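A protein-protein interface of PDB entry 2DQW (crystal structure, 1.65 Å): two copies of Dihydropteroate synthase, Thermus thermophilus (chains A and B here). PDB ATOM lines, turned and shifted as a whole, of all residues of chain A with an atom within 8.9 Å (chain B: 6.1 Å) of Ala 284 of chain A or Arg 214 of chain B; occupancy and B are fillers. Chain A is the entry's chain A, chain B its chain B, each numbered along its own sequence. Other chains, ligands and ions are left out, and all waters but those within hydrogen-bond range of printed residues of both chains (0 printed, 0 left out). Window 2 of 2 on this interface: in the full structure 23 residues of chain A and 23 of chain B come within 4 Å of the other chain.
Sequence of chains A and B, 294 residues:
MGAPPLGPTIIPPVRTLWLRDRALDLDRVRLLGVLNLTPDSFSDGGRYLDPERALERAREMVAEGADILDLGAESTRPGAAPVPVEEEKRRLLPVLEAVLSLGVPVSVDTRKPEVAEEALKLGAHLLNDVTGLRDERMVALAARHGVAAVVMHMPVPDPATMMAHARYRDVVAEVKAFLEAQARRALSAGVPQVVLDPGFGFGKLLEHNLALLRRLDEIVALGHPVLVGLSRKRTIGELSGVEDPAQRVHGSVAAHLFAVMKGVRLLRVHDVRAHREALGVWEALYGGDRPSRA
NZ of Lys 262 of chain B sits at hydrogen-bond distance from O of Arg 214 of chain B, 3.0 Å away.
O of Ala 284 of chain A sits at hydrogen-bond distance from NH2 of Arg 214 of chain B, 2.5 Å away.
NE of Arg 214 of chain B lies within hydrogen-bond range of O of Leu 285 of chain A.
Among the printed residues, merely in contact across the chains: Gly 280 of chain A with Leu 239 of chain B, Leu 285 of chain A with Leu 213 of chain B, Leu 285 of chain A with Leu 210 of chain B, Ala 284 of chain A with Leu 239 of chain B, Trp 282 of chain A with Phe 258 of chain B, Tyr 286 of chain A with Phe 258 of chain B, Leu 285 of chain A with Phe 258 of chain B and Val 281 of chain A with Leu 239 of chain B.
No position is printed for both chains.
Of the 10 pairs that touch across the chains among the printed residues, none has its exchanged pair printed and touching as well.
Hydrophobic or aromatic side chains of chain B within 4 Å of the printed part of chain A: Leu 210, Leu 213, Leu 239 and Phe 258.
Of the 13 printed residues of chain A, 6 touch a printed residue of chain B.
Along chain A the printed residues that touch a printed residue of chain B span positions 280 to 286.
Among the printed residues, no Asp or Glu carboxylate lies within 4 Å of a Lys or Arg side-chain nitrogen of the other chain.
Of the printed residues of chain B, Val 281 of chain A touches Leu 239.
Printed residues of chain B within 4 Å of Trp 282 of chain A: Phe 258 (3.7 Å).
Of chain B, only Arg 214 and Leu 239 come within 4 Å of Ala 284 of chain A.
Printed residues of chain B within 4 Å of Leu 285 of chain A: Leu 210 (3.5 Å), Leu 213 (3.5 Å), Arg 214 (3.4 Å) and Phe 258 (3.7 Å).
Printed residues of chain A within 4 Å of Leu 210 of chain B: Leu 285 (3.5 Å).
Ala 211 of chain B touches none of the printed residues of chain A.
Arg 214 of chain B touches two residues of chain A.
Printed residues of chain A within 4 Å of Phe 258 of chain B: Trp 282, Leu 285 and Tyr 286.
The nearest printed residue of chain A that does not touch Leu 213 of chain B is Val 281 of chain A (6.2 Å).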
ATOM      1  N   ARG A  28      13.234  27.298  13.161  1.00  0.00           N
ATOM      2  CA  ARG A  28      13.280  25.850  13.255  1.00  0.00           C
ATOM      3  C   ARG A  28      13.048  25.540  14.723  1.00  0.00           C
ATOM      4  O   ARG A  28      13.204  26.406  15.585  1.00  0.00           O
ATOM      5  CB  ARG A  28      14.640  25.311  12.799  1.00  0.00           C
ATOM      6  CG  ARG A  28      15.817  25.739  13.660  1.00  0.00           C
ATOM      7  CD  ARG A  28      17.144  25.598  12.911  1.00  0.00           C
ATOM      8  NE  ARG A  28      17.477  24.217  12.567  1.00  0.00           N
ATOM      9  CZ  ARG A  28      17.902  23.304  13.436  1.00  0.00           C
ATOM     10  NH1 ARG A  28      18.049  23.616  14.716  1.00  0.00           N
ATOM     11  NH2 ARG A  28      18.192  22.077  13.022  1.00  0.00           N
ATOM     12  N   ARG A 276      16.618  15.594  18.173  1.00  0.00           N
ATOM     13  CA  ARG A 276      17.395  16.216  17.099  1.00  0.00           C
ATOM     14  C   ARG A 276      17.360  15.313  15.869  1.00  0.00           C
ATOM     15  O   ARG A 276      17.191  15.784  14.746  1.00  0.00           O
ATOM     16  CB  ARG A 276      18.838  16.465  17.553  1.00  0.00           C
ATOM     17  CG  ARG A 276      19.016  17.791  18.302  1.00  0.00           C
ATOM     18  CD  ARG A 276      19.147  18.960  17.324  1.00  0.00           C
ATOM     19  NE  ARG A 276      18.653  20.230  17.862  1.00  0.00           N
ATOM     20  CZ  ARG A 276      17.610  20.888  17.362  1.00  0.00           C
ATOM     21  NH1 ARG A 276      16.954  20.396  16.315  1.00  0.00           N
ATOM     22  NH2 ARG A 276      17.225  22.038  17.900  1.00  0.00           N
ATOM     23  N   GLU A 277      17.509  14.008  16.084  1.00  0.00           N
ATOM     24  CA  GLU A 277      17.466  13.056  14.979  1.00  0.00           C
ATOM     25  C   GLU A 277      16.097  13.044  14.293  1.00  0.00           C
ATOM     26  O   GLU A 277      16.004  13.065  13.064  1.00  0.00           O
ATOM     27  CB  GLU A 277      17.822  11.657  15.493  1.00  0.00           C
ATOM     28  CG  GLU A 277      19.303  11.548  15.831  1.00  0.00           C
ATOM     29  CD  GLU A 277      19.660  10.346  16.681  1.00  0.00           C
ATOM     30  OE1 GLU A 277      18.787   9.501  16.946  1.00  0.00           O
ATOM     31  OE2 GLU A 277      20.841  10.258  17.084  1.00  0.00           O
ATOM     32  N   ALA A 278      15.033  13.009  15.087  1.00  0.00           N
ATOM     33  CA  ALA A 278      13.687  12.996  14.528  1.00  0.00           C
ATOM     34  C   ALA A 278      13.388  14.297  13.783  1.00  0.00           C
ATOM     35  O   ALA A 278      12.807  14.270  12.699  1.00  0.00           O
ATOM     36  CB  ALA A 278      12.645  12.783  15.644  1.00  0.00           C
ATOM     37  N   LEU A 279      13.774  15.429  14.363  1.00  0.00           N
ATOM     38  CA  LEU A 279      13.525  16.720  13.728  1.00  0.00           C
ATOM     39  C   LEU A 279      14.310  16.886  12.439  1.00  0.00           C
ATOM     40  O   LEU A 279      13.843  17.543  11.510  1.00  0.00           O
ATOM     41  CB  LEU A 279      13.848  17.871  14.688  1.00  0.00           C
ATOM     42  CG  LEU A 279      12.855  18.025  15.847  1.00  0.00           C
ATOM     43  CD1 LEU A 279      13.435  18.952  16.900  1.00  0.00           C
ATOM     44  CD2 LEU A 279      11.513  18.554  15.326  1.00  0.00           C
ATOM     45  N   GLY A 280      15.495  16.280  12.378  1.00  0.00           N
ATOM     46  CA  GLY A 280      16.296  16.388  11.170  1.00  0.00           C
ATOM     47  C   GLY A 280      15.494  15.890   9.987  1.00  0.00           C
ATOM     48  O   GLY A 280      15.539  16.455   8.887  1.00  0.00           O
ATOM     49  N   VAL A 281      14.757  14.809  10.209  1.00  0.00           N
ATOM     50  CA  VAL A 281      13.921  14.237   9.177  1.00  0.00           C
ATOM     51  C   VAL A 281      12.649  15.064   9.012  1.00  0.00           C
ATOM     52  O   VAL A 281      12.330  15.529   7.920  1.00  0.00           O
ATOM     53  CB  VAL A 281      13.518  12.779   9.524  1.00  0.00           C
ATOM     54  CG1 VAL A 281      12.464  12.271   8.545  1.00  0.00           C
ATOM     55  CG2 VAL A 281      14.745  11.882   9.484  1.00  0.00           C
ATOM     56  N   TRP A 282      11.936  15.266  10.113  1.00  0.00           N
ATOM     57  CA  TRP A 282      10.670  15.988  10.048  1.00  0.00           C
ATOM     58  C   TRP A 282      10.749  17.366   9.406  1.00  0.00           C
ATOM     59  O   TRP A 282       9.964  17.688   8.506  1.00  0.00           O
ATOM     60  CB  TRP A 282      10.066  16.105  11.451  1.00  0.00           C
ATOM     61  CG  TRP A 282       8.651  16.585  11.428  1.00  0.00           C
ATOM     62  CD1 TRP A 282       8.214  17.877  11.525  1.00  0.00           C
ATOM     63  CD2 TRP A 282       7.487  15.775  11.244  1.00  0.00           C
ATOM     64  NE1 TRP A 282       6.840  17.918  11.412  1.00  0.00           N
ATOM     65  CE2 TRP A 282       6.372  16.641  11.237  1.00  0.00           C
ATOM     66  CE3 TRP A 282       7.279  14.399  11.081  1.00  0.00           C
ATOM     67  CZ2 TRP A 282       5.062  16.174  11.074  1.00  0.00           C
ATOM     68  CZ3 TRP A 282       5.981  13.932  10.920  1.00  0.00           C
ATOM     69  CH2 TRP A 282       4.887  14.820  10.917  1.00  0.00           C
ATOM     70  N   GLU A 283      11.701  18.173   9.846  1.00  0.00           N
ATOM     71  CA  GLU A 283      11.823  19.526   9.315  1.00  0.00           C
ATOM     72  C   GLU A 283      12.292  19.572   7.870  1.00  0.00           C
ATOM     73  O   GLU A 283      12.030  20.540   7.157  1.00  0.00           O
ATOM     74  CB  GLU A 283      12.728  20.361  10.217  1.00  0.00           C
ATOM     75  CG  GLU A 283      12.121  20.577  11.598  1.00  0.00           C
ATOM     76  CD  GLU A 283      12.940  21.497  12.469  1.00  0.00           C
ATOM     77  OE1 GLU A 283      14.082  21.139  12.816  1.00  0.00           O
ATOM     78  OE2 GLU A 283      12.440  22.586  12.808  1.00  0.00           O
ATOM     79  N   ALA A 284      12.980  18.528   7.429  1.00  0.00           N
ATOM     80  CA  ALA A 284      13.433  18.487   6.044  1.00  0.00           C
ATOM     81  C   ALA A 284      12.232  18.176   5.154  1.00  0.00           C
ATOM     82  O   ALA A 284      12.104  18.715   4.056  1.00  0.00           O
ATOM     83  CB  ALA A 284      14.515  17.420   5.869  1.00  0.00           C
ATOM     84  N   LEU A 285      11.346  17.312   5.641  1.00  0.00           N
ATOM     85  CA  LEU A 285      10.153  16.919   4.894  1.00  0.00           C
ATOM     86  C   LEU A 285       9.078  17.992   4.926  1.00  0.00           C
ATOM     87  O   LEU A 285       8.748  18.595   3.900  1.00  0.00           O
ATOM     88  CB  LEU A 285       9.572  15.624   5.463  1.00  0.00           C
ATOM     89  CG  LEU A 285      10.452  14.382   5.342  1.00  0.00           C
ATOM     90  CD1 LEU A 285       9.787  13.201   6.025  1.00  0.00           C
ATOM     91  CD2 LEU A 285      10.695  14.085   3.869  1.00  0.00           C
ATOM     92  N   TYR A 286       8.530  18.208   6.118  1.00  0.00           N
ATOM     93  CA  TYR A 286       7.480  19.191   6.345  1.00  0.00           C
ATOM     94  C   TYR A 286       8.123  20.572   6.337  1.00  0.00           C
ATOM     95  O   TYR A 286       8.105  21.282   7.342  1.00  0.00           O
ATOM     96  CB  TYR A 286       6.818  18.916   7.699  1.00  0.00           C
ATOM     97  CG  TYR A 286       5.413  19.451   7.856  1.00  0.00           C
ATOM     98  CD1 TYR A 286       4.378  18.612   8.272  1.00  0.00           C
ATOM     99  CD2 TYR A 286       5.119  20.794   7.624  1.00  0.00           C
ATOM    100  CE1 TYR A 286       3.087  19.097   8.458  1.00  0.00           C
ATOM    101  CE2 TYR A 286       3.826  21.291   7.809  1.00  0.00           C
ATOM    102  CZ  TYR A 286       2.816  20.435   8.226  1.00  0.00           C
ATOM    103  OH  TYR A 286       1.540  20.917   8.421  1.00  0.00           O
ATOM    104  N   GLY A 287       8.703  20.935   5.197  1.00  0.00           N
ATOM    105  CA  GLY A 287       9.357  22.224   5.071  1.00  0.00           C
ATOM    106  C   GLY A 287      10.590  22.150   4.191  1.00  0.00           C
ATOM    107  O   GLY A 287      11.702  22.402   4.698  1.00  0.00           O
ATOM    108  N   GLU B 207      17.391  13.816  -2.973  1.00  0.00           N
ATOM    109  CA  GLU B 207      16.428  14.724  -3.597  1.00  0.00           C
ATOM    110  C   GLU B 207      15.199  13.991  -4.125  1.00  0.00           C
ATOM    111  O   GLU B 207      14.079  14.506  -4.037  1.00  0.00           O
ATOM    112  CB  GLU B 207      17.098  15.516  -4.728  1.00  0.00           C
ATOM    113  CG  GLU B 207      17.852  14.660  -5.729  1.00  0.00           C
ATOM    114  CD  GLU B 207      18.859  15.462  -6.537  1.00  0.00           C
ATOM    115  OE1 GLU B 207      18.445  16.197  -7.459  1.00  0.00           O
ATOM    116  OE2 GLU B 207      20.069  15.365  -6.239  1.00  0.00           O
ATOM    117  N   ASN B 209      14.070  10.932  -3.036  1.00  0.00           N
ATOM    118  CA  ASN B 209      13.322  10.389  -1.912  1.00  0.00           C
ATOM    119  C   ASN B 209      12.527  11.485  -1.205  1.00  0.00           C
ATOM    120  O   ASN B 209      11.399  11.254  -0.755  1.00  0.00           O
ATOM    121  CB  ASN B 209      14.277   9.688  -0.939  1.00  0.00           C
ATOM    122  CG  ASN B 209      14.881   8.440  -1.537  1.00  0.00           C
ATOM    123  OD1 ASN B 209      14.163   7.536  -1.947  1.00  0.00           O
ATOM    124  ND2 ASN B 209      16.209   8.385  -1.599  1.00  0.00           N
ATOM    125  N   LEU B 210      13.103  12.679  -1.118  1.00  0.00           N
ATOM    126  CA  LEU B 210      12.414  13.794  -0.475  1.00  0.00           C
ATOM    127  C   LEU B 210      11.189  14.191  -1.285  1.00  0.00           C
ATOM    128  O   LEU B 210      10.115  14.419  -0.731  1.00  0.00           O
ATOM    129  CB  LEU B 210      13.335  15.009  -0.345  1.00  0.00           C
ATOM    130  CG  LEU B 210      14.339  14.993   0.807  1.00  0.00           C
ATOM    131  CD1 LEU B 210      15.242  16.218   0.703  1.00  0.00           C
ATOM    132  CD2 LEU B 210      13.595  14.986   2.139  1.00  0.00           C
ATOM    133  N   ALA B 211      11.363  14.277  -2.599  1.00  0.00           N
ATOM    134  CA  ALA B 211      10.271  14.661  -3.485  1.00  0.00           C
ATOM    135  C   ALA B 211       9.114  13.675  -3.382  1.00  0.00           C
ATOM    136  O   ALA B 211       7.949  14.078  -3.313  1.00  0.00           O
ATOM    137  CB  ALA B 211      10.775  14.738  -4.929  1.00  0.00           C
ATOM    138  N   LEU B 212       9.432  12.383  -3.380  1.00  0.00           N
ATOM    139  CA  LEU B 212       8.410  11.346  -3.287  1.00  0.00           C
ATOM    140  C   LEU B 212       7.667  11.400  -1.959  1.00  0.00           C
ATOM    141  O   LEU B 212       6.449  11.244  -1.918  1.00  0.00           O
ATOM    142  CB  LEU B 212       9.037   9.965  -3.487  1.00  0.00           C
ATOM    143  CG  LEU B 212       9.385   9.625  -4.940  1.00  0.00           C
ATOM    144  CD1 LEU B 212      10.383   8.479  -4.984  1.00  0.00           C
ATOM    145  CD2 LEU B 212       8.109   9.257  -5.681  1.00  0.00           C
ATOM    146  N   LEU B 213       8.396  11.631  -0.873  1.00  0.00           N
ATOM    147  CA  LEU B 213       7.761  11.715   0.439  1.00  0.00           C
ATOM    148  C   LEU B 213       6.825  12.916   0.530  1.00  0.00           C
ATOM    149  O   LEU B 213       5.698  12.798   1.018  1.00  0.00           O
ATOM    150  CB  LEU B 213       8.827  11.817   1.534  1.00  0.00           C
ATOM    151  CG  LEU B 213       9.491  10.507   1.947  1.00  0.00           C
ATOM    152  CD1 LEU B 213      10.769  10.804   2.712  1.00  0.00           C
ATOM    153  CD2 LEU B 213       8.524   9.694   2.798  1.00  0.00           C
ATOM    154  N   ARG B 214       7.291  14.066   0.052  1.00  0.00           N
ATOM    155  CA  ARG B 214       6.498  15.292   0.096  1.00  0.00           C
ATOM    156  C   ARG B 214       5.221  15.216  -0.729  1.00  0.00           C
ATOM    157  O   ARG B 214       4.246  15.903  -0.437  1.00  0.00           O
ATOM    158  CB  ARG B 214       7.343  16.478  -0.360  1.00  0.00           C
ATOM    159  CG  ARG B 214       8.412  16.886   0.652  1.00  0.00           C
ATOM    160  CD  ARG B 214       9.386  17.876   0.050  1.00  0.00           C
ATOM    161  NE  ARG B 214      10.409  18.287   1.007  1.00  0.00           N
ATOM    162  CZ  ARG B 214      11.576  18.823   0.663  1.00  0.00           C
ATOM    163  NH1 ARG B 214      11.871  19.013  -0.618  1.00  0.00           N
ATOM    164  NH2 ARG B 214      12.452  19.170   1.595  1.00  0.00           N
ATOM    165  N   ARG B 215       5.220  14.382  -1.761  1.00  0.00           N
ATOM    166  CA  ARG B 215       4.032  14.239  -2.597  1.00  0.00           C
ATOM    167  C   ARG B 215       3.459  12.826  -2.514  1.00  0.00           C
ATOM    168  O   ARG B 215       2.765  12.363  -3.425  1.00  0.00           O
ATOM    169  CB  ARG B 215       4.366  14.604  -4.050  1.00  0.00           C
ATOM    170  CG  ARG B 215       4.675  16.082  -4.248  1.00  0.00           C
ATOM    171  CD  ARG B 215       5.174  16.369  -5.652  1.00  0.00           C
ATOM    172  NE  ARG B 215       4.172  16.052  -6.665  1.00  0.00           N
ATOM    173  CZ  ARG B 215       4.400  16.090  -7.975  1.00  0.00           C
ATOM    174  NH1 ARG B 215       5.597  16.430  -8.434  1.00  0.00           N
ATOM    175  NH2 ARG B 215       3.429  15.789  -8.825  1.00  0.00           N
ATOM    176  N   LEU B 216       3.725  12.150  -1.401  1.00  0.00           N
ATOM    177  CA  LEU B 216       3.250  10.791  -1.204  1.00  0.00           C
ATOM    178  C   LEU B 216       1.724  10.687  -1.285  1.00  0.00           C
ATOM    179  O   LEU B 216       1.188   9.651  -1.669  1.00  0.00           O
ATOM    180  CB  LEU B 216       3.756  10.262   0.145  1.00  0.00           C
ATOM    181  CG  LEU B 216       3.660   8.760   0.406  1.00  0.00           C
ATOM    182  CD1 LEU B 216       4.346   7.984  -0.713  1.00  0.00           C
ATOM    183  CD2 LEU B 216       4.308   8.448   1.752  1.00  0.00           C
ATOM    184  N   ASP B 217       1.033  11.766  -0.933  1.00  0.00           N
ATOM    185  CA  ASP B 217      -0.426  11.784  -0.986  1.00  0.00           C
ATOM    186  C   ASP B 217      -0.917  11.506  -2.404  1.00  0.00           C
ATOM    187  O   ASP B 217      -1.997  10.944  -2.593  1.00  0.00           O
ATOM    188  CB  ASP B 217      -0.949  13.144  -0.510  1.00  0.00           C
ATOM    189  CG  ASP B 217      -0.265  14.306  -1.204  1.00  0.00           C
ATOM    190  OD1 ASP B 217       0.961  14.465  -1.040  1.00  0.00           O
ATOM    191  OD2 ASP B 217      -0.948  15.070  -1.920  1.00  0.00           O
ATOM    192  N   LEU B 239      19.365  12.676   6.645  1.00  0.00           N
ATOM    193  CA  LEU B 239      18.592  13.734   7.288  1.00  0.00           C
ATOM    194  C   LEU B 239      18.754  13.843   8.796  1.00  0.00           C
ATOM    195  O   LEU B 239      18.680  14.943   9.339  1.00  0.00           O
ATOM    196  CB  LEU B 239      17.111  13.578   6.945  1.00  0.00           C
ATOM    197  CG  LEU B 239      16.776  13.689   5.453  1.00  0.00           C
ATOM    198  CD1 LEU B 239      15.295  13.415   5.256  1.00  0.00           C
ATOM    199  CD2 LEU B 239      17.142  15.071   4.926  1.00  0.00           C
ATOM    200  N   PHE B 258       5.317  10.838   9.095  1.00  0.00           N
ATOM    201  CA  PHE B 258       5.025  11.781   8.022  1.00  0.00           C
ATOM    202  C   PHE B 258       4.273  11.040   6.915  1.00  0.00           C
ATOM    203  O   PHE B 258       3.307  11.563   6.367  1.00  0.00           O
ATOM    204  CB  PHE B 258       6.323  12.399   7.483  1.00  0.00           C
ATOM    205  CG  PHE B 258       6.108  13.440   6.414  1.00  0.00           C
ATOM    206  CD1 PHE B 258       5.990  13.074   5.075  1.00  0.00           C
ATOM    207  CD2 PHE B 258       6.026  14.788   6.748  1.00  0.00           C
ATOM    208  CE1 PHE B 258       5.804  14.038   4.085  1.00  0.00           C
ATOM    209  CE2 PHE B 258       5.838  15.761   5.769  1.00  0.00           C
ATOM    210  CZ  PHE B 258       5.726  15.382   4.429  1.00  0.00           C
ATOM    211  N   LYS B 262       0.424  11.483   5.409  1.00  0.00           N
ATOM    212  CA  LYS B 262       0.127  11.569   3.974  1.00  0.00           C
ATOM    213  C   LYS B 262      -0.893  10.531   3.512  1.00  0.00           C
ATOM    214  O   LYS B 262      -1.298  10.526   2.345  1.00  0.00           O
ATOM    215  CB  LYS B 262       1.416  11.411   3.152  1.00  0.00           C
ATOM    216  CG  LYS B 262       2.343  12.615   3.200  1.00  0.00           C
ATOM    217  CD  LYS B 262       1.713  13.808   2.503  1.00  0.00           C
ATOM    218  CE  LYS B 262       2.653  14.995   2.476  1.00  0.00           C
ATOM    219  NZ  LYS B 262       2.079  16.104   1.660  1.00  0.00           N
